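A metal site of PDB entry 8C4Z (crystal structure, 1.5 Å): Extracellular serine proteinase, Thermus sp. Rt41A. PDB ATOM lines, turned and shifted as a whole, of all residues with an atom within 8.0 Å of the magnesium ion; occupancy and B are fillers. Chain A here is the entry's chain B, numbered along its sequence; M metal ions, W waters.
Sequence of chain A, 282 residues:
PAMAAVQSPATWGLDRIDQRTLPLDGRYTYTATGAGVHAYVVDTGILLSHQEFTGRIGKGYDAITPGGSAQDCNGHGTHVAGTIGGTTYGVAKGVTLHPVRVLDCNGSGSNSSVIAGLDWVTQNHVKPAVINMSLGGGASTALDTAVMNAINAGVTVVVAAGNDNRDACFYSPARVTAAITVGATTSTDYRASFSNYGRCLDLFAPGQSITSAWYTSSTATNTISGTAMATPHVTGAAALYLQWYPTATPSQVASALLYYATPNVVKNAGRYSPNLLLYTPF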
ATOM      1  N   ILE A 151     -18.288  13.549  16.061  1.00  0.00           N
ATOM      2  CA  ILE A 151     -19.682  13.578  16.512  1.00  0.00           C
ATOM      3  C   ILE A 151     -20.643  13.365  15.340  1.00  0.00           C
ATOM      4  O   ILE A 151     -21.649  12.649  15.460  1.00  0.00           O
ATOM      5  CB  ILE A 151     -19.948  14.894  17.264  1.00  0.00           C
ATOM      6  CG1 ILE A 151     -19.104  14.946  18.525  1.00  0.00           C
ATOM      7  CG2 ILE A 151     -21.448  15.054  17.570  1.00  0.00           C
ATOM      8  CD1 ILE A 151     -19.037  16.314  19.162  1.00  0.00           C
ATOM      9  N   VAL A 157     -18.590  12.328  22.038  1.00  0.00           N
ATOM     10  CA  VAL A 157     -17.270  12.786  22.467  1.00  0.00           C
ATOM     11  C   VAL A 157     -17.416  13.486  23.808  1.00  0.00           C
ATOM     12  O   VAL A 157     -18.126  14.496  23.903  1.00  0.00           O
ATOM     13  CB  VAL A 157     -16.604  13.722  21.451  1.00  0.00           C
ATOM     14  CG1 VAL A 157     -15.243  14.164  21.975  1.00  0.00           C
ATOM     15  CG2 VAL A 157     -16.487  13.048  20.092  1.00  0.00           C
ATOM     16  N   VAL A 159     -15.359  15.394  26.869  1.00  0.00           N
ATOM     17  CA  VAL A 159     -14.118  16.160  26.982  1.00  0.00           C
ATOM     18  C   VAL A 159     -14.018  16.845  28.343  1.00  0.00           C
ATOM     19  O   VAL A 159     -15.021  17.246  28.937  1.00  0.00           O
ATOM     20  CB  VAL A 159     -13.944  17.202  25.839  1.00  0.00           C
ATOM     21  CG1 VAL A 159     -14.117  16.556  24.480  1.00  0.00           C
ATOM     22  CG2 VAL A 159     -14.930  18.368  25.979  1.00  0.00           C
ATOM     23  N   PRO A 173     -10.605  21.029  23.274  1.00  0.00           N
ATOM     24  CA  PRO A 173     -11.934  21.004  22.655  1.00  0.00           C
ATOM     25  C   PRO A 173     -13.074  21.355  23.630  1.00  0.00           C
ATOM     26  O   PRO A 173     -14.225  21.127  23.277  1.00  0.00           O
ATOM     27  CB  PRO A 173     -12.072  19.549  22.200  1.00  0.00           C
ATOM     28  CG  PRO A 173     -11.265  18.781  23.236  1.00  0.00           C
ATOM     29  CD  PRO A 173     -10.118  19.676  23.604  1.00  0.00           C
ATOM     30  N   ALA A 174     -12.758  21.895  24.821  1.00  0.00           N
ATOM     31  CA  ALA A 174     -13.806  22.142  25.805  1.00  0.00           C
ATOM     32  C   ALA A 174     -14.915  23.040  25.264  1.00  0.00           C
ATOM     33  O   ALA A 174     -16.093  22.852  25.601  1.00  0.00           O
ATOM     34  CB  ALA A 174     -13.222  22.724  27.096  1.00  0.00           C
ATOM     35  N   ARG A 175     -14.573  23.986  24.394  1.00  0.00           N
ATOM     36  CA  ARG A 175     -15.544  24.940  23.865  1.00  0.00           C
ATOM     37  C   ARG A 175     -16.456  24.361  22.786  1.00  0.00           C
ATOM     38  O   ARG A 175     -17.371  25.058  22.339  1.00  0.00           O
ATOM     39  CB  ARG A 175     -14.849  26.196  23.309  1.00  0.00           C
ATOM     40  CG  ARG A 175     -14.037  25.962  22.041  1.00  0.00           C
ATOM     41  CD  ARG A 175     -13.305  27.224  21.578  1.00  0.00           C
ATOM     42  NE  ARG A 175     -12.677  27.002  20.273  1.00  0.00           N
ATOM     43  CZ  ARG A 175     -12.144  27.958  19.521  1.00  0.00           C
ATOM     44  NH1 ARG A 175     -12.173  29.229  19.899  1.00  0.00           N
ATOM     45  NH2 ARG A 175     -11.571  27.630  18.367  1.00  0.00           N
ATOM     46  N   VAL A 176     -16.248  23.110  22.361  1.00  0.00           N
ATOM     47  CA  VAL A 176     -17.080  22.526  21.302  1.00  0.00           C
ATOM     48  C   VAL A 176     -18.448  22.177  21.881  1.00  0.00           C
ATOM     49  O   VAL A 176     -18.570  21.250  22.686  1.00  0.00           O
ATOM     50  CB  VAL A 176     -16.405  21.318  20.656  1.00  0.00           C
ATOM     51  CG1 VAL A 176     -17.311  20.712  19.572  1.00  0.00           C
ATOM     52  CG2 VAL A 176     -15.035  21.701  20.057  1.00  0.00           C
ATOM     53  N   THR A 177     -19.490  22.910  21.462  1.00  0.00           N
ATOM     54  CA  THR A 177     -20.831  22.769  22.044  1.00  0.00           C
ATOM     55  C   THR A 177     -21.337  21.328  21.978  1.00  0.00           C
ATOM     56  O   THR A 177     -21.899  20.816  22.957  1.00  0.00           O
ATOM     57  CB  THR A 177     -21.789  23.685  21.288  1.00  0.00           C
ATOM     58  OG1 THR A 177     -21.319  25.036  21.376  1.00  0.00           O
ATOM     59  CG2 THR A 177     -23.189  23.601  21.883  1.00  0.00           C
ATOM     60  N   ALA A 178     -21.162  20.675  20.841  1.00  0.00           N
ATOM     61  CA  ALA A 178     -21.753  19.348  20.663  1.00  0.00           C
ATOM     62  C   ALA A 178     -21.034  18.264  21.462  1.00  0.00           C
ATOM     63  O   ALA A 178     -21.573  17.160  21.597  1.00  0.00           O
ATOM     64  CB  ALA A 178     -21.799  19.008  19.184  1.00  0.00           C
ATOM     65  N   ALA A 179     -19.832  18.540  21.965  1.00  0.00           N
ATOM     66  CA  ALA A 179     -19.178  17.597  22.861  1.00  0.00           C
ATOM     67  C   ALA A 179     -19.759  17.758  24.266  1.00  0.00           C
ATOM     68  O   ALA A 179     -20.310  18.803  24.600  1.00  0.00           O
ATOM     69  CB  ALA A 179     -17.676  17.865  22.899  1.00  0.00           C
ATOM     70  N   ILE A 180     -19.661  16.702  25.071  1.00  0.00           N
ATOM     71  CA  ILE A 180     -20.110  16.767  26.462  1.00  0.00           C
ATOM     72  C   ILE A 180     -18.905  17.216  27.284  1.00  0.00           C
ATOM     73  O   ILE A 180     -17.940  16.466  27.444  1.00  0.00           O
ATOM     74  CB  ILE A 180     -20.643  15.398  26.940  1.00  0.00           C
ATOM     75  CG1 ILE A 180     -21.821  14.958  26.075  1.00  0.00           C
ATOM     76  CG2 ILE A 180     -21.059  15.470  28.407  1.00  0.00           C
ATOM     77  CD1 ILE A 180     -22.293  13.556  26.361  1.00  0.00           C
ATOM     78  N   THR A 181     -18.943  18.458  27.752  1.00  0.00           N
ATOM     79  CA  THR A 181     -17.819  19.066  28.461  1.00  0.00           C
ATOM     80  C   THR A 181     -18.065  18.923  29.955  1.00  0.00           C
ATOM     81  O   THR A 181     -19.119  19.331  30.455  1.00  0.00           O
ATOM     82  CB  THR A 181     -17.667  20.541  28.068  1.00  0.00           C
ATOM     83  OG1 THR A 181     -17.477  20.629  26.655  1.00  0.00           O
ATOM     84  CG2 THR A 181     -16.473  21.190  28.776  1.00  0.00           C
ATOM     85  N   VAL A 182     -17.078  18.375  30.668  1.00  0.00           N
ATOM     86  CA  VAL A 182     -17.264  17.888  32.031  1.00  0.00           C
ATOM     87  C   VAL A 182     -16.379  18.675  33.007  1.00  0.00           C
ATOM     88  O   VAL A 182     -15.154  18.667  32.877  1.00  0.00           O
ATOM     89  CB  VAL A 182     -16.952  16.389  32.129  1.00  0.00           C
ATOM     90  CG1 VAL A 182     -17.264  15.889  33.536  1.00  0.00           C
ATOM     91  CG2 VAL A 182     -17.764  15.633  31.094  1.00  0.00           C
ATOM     92  N   ARG A 199     -20.605  28.568  30.634  1.00  0.00           N
ATOM     93  CA  ARG A 199     -21.688  28.152  29.740  1.00  0.00           C
ATOM     94  C   ARG A 199     -21.283  27.006  28.815  1.00  0.00           C
ATOM     95  O   ARG A 199     -22.157  26.346  28.241  1.00  0.00           O
ATOM     96  CB  ARG A 199     -22.163  29.333  28.894  1.00  0.00           C
ATOM     97  CG  ARG A 199     -21.102  29.860  27.971  1.00  0.00           C
ATOM     98  CD  ARG A 199     -21.605  30.984  27.082  1.00  0.00           C
ATOM     99  NE  ARG A 199     -20.491  31.835  26.668  1.00  0.00           N
ATOM    100  CZ  ARG A 199     -19.891  31.772  25.495  1.00  0.00           C
ATOM    101  NH1 ARG A 199     -20.266  30.883  24.575  1.00  0.00           N
ATOM    102  NH2 ARG A 199     -18.880  32.593  25.238  1.00  0.00           N
ATOM    103  N   CYS A 200     -19.985  26.750  28.643  1.00  0.00           N
ATOM    104  CA  CYS A 200     -19.538  25.671  27.777  1.00  0.00           C
ATOM    105  C   CYS A 200     -19.557  24.311  28.464  1.00  0.00           C
ATOM    106  O   CYS A 200     -19.485  23.291  27.764  1.00  0.00           O
ATOM    107  CB  CYS A 200     -18.164  25.981  27.173  1.00  0.00           C
ATOM    108  SG  CYS A 200     -18.152  27.262  25.866  1.00  0.00           S
ATOM    109  N   LEU A 201     -19.677  24.274  29.792  1.00  0.00           N
ATOM    110  CA  LEU A 201     -19.838  22.998  30.469  1.00  0.00           C
ATOM    111  C   LEU A 201     -21.213  22.416  30.201  1.00  0.00           C
ATOM    112  O   LEU A 201     -22.190  23.131  29.980  1.00  0.00           O
ATOM    113  CB  LEU A 201     -19.684  23.135  31.987  1.00  0.00           C
ATOM    114  CG  LEU A 201     -18.280  22.998  32.576  1.00  0.00           C
ATOM    115  CD1 LEU A 201     -17.349  24.046  31.961  1.00  0.00           C
ATOM    116  CD2 LEU A 201     -18.337  23.121  34.108  1.00  0.00           C
ATOM    117  N   ASP A 202     -21.284  21.096  30.249  1.00  0.00           N
ATOM    118  CA  ASP A 202     -22.570  20.391  30.218  1.00  0.00           C
ATOM    119  C   ASP A 202     -22.993  19.913  31.593  1.00  0.00           C
ATOM    120  O   ASP A 202     -24.165  20.056  31.962  1.00  0.00           O
ATOM    121  CB  ASP A 202     -22.454  19.218  29.237  1.00  0.00           C
ATOM    122  CG  ASP A 202     -22.540  19.680  27.801  1.00  0.00           C
ATOM    123  OD1 ASP A 202     -23.631  20.096  27.370  1.00  0.00           O
ATOM    124  OD2 ASP A 202     -21.485  19.727  27.128  1.00  0.00           O
ATOM    125  N   LEU A 203     -22.052  19.389  32.383  1.00  0.00           N
ATOM    126  CA  LEU A 203     -22.345  18.921  33.729  1.00  0.00           C
ATOM    127  C   LEU A 203     -21.034  18.706  34.472  1.00  0.00           C
ATOM    128  O   LEU A 203     -19.938  18.866  33.918  1.00  0.00           O
ATOM    129  CB  LEU A 203     -23.185  17.635  33.717  1.00  0.00           C
ATOM    130  CG  LEU A 203     -22.501  16.322  33.332  1.00  0.00           C
ATOM    131  CD1 LEU A 203     -23.500  15.207  33.582  1.00  0.00           C
ATOM    132  CD2 LEU A 203     -22.045  16.302  31.880  1.00  0.00           C
ATOM    133  N   ALA A 254     -26.456  12.759  25.054  1.00  0.00           N
ATOM    134  CA  ALA A 254     -26.326  13.954  25.880  1.00  0.00           C
ATOM    135  C   ALA A 254     -27.662  14.333  26.521  1.00  0.00           C
ATOM    136  O   ALA A 254     -27.712  14.632  27.719  1.00  0.00           O
ATOM    137  CB  ALA A 254     -25.769  15.101  25.038  1.00  0.00           C
ATOM    138  N   LEU A 258     -28.213  14.515  30.574  1.00  0.00           N
ATOM    139  CA  LEU A 258     -28.602  15.780  31.166  1.00  0.00           C
ATOM    140  C   LEU A 258     -29.973  15.697  31.825  1.00  0.00           C
ATOM    141  O   LEU A 258     -30.201  16.328  32.858  1.00  0.00           O
ATOM    142  CB  LEU A 258     -28.532  16.913  30.131  1.00  0.00           C
ATOM    143  CG  LEU A 258     -27.122  17.148  29.579  1.00  0.00           C
ATOM    144  CD1 LEU A 258     -27.127  18.187  28.474  1.00  0.00           C
ATOM    145  CD2 LEU A 258     -26.202  17.561  30.711  1.00  0.00           C
HETATM  146 MG    MG M   1     -21.769  20.312  25.106  1.00  0.00          MG
HETATM  147  O   HOH W   1     -22.629  22.090  25.477  1.00  0.00           O
HETATM  148  O   HOH W   2     -23.386  18.965  24.769  1.00  0.00           O
HETATM  149  O   HOH W   3     -19.724  21.094  25.228  1.00  0.00           O
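The backbone NH (N) of Asp 202 sits at hydrogen-bond distance from the backbone carbonyl oxygen (O) of Thr 181.
Of the 20 residues printed, 3 come within 4 Å of the magnesium ion. The nearest printed residue that does not touch the magnesium ion is Val 176 (4.1 Å).
Water W1 is bound to the magnesium ion. OD2 of Asp 202 binds the magnesium ion, 2.1 Å away. Water W2 binds the magnesium ion (2.1 Å). The backbone carbonyl oxygen (O) of Ala 179 binds the magnesium ion, 2.2 Å away. Water W3 is bound to the magnesium ion (2.2 Å). O of Thr 177 binds the magnesium ion, 2.2 Å away.
Water W3 lies within hydrogen-bond range of the side-chain hydroxyl of Thr 181 (2.7 Å), the backbone carbonyl oxygen of Val 176 (2.8 Å) and the backbone carbonyl oxygen of Cys 200 (3.4 Å).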
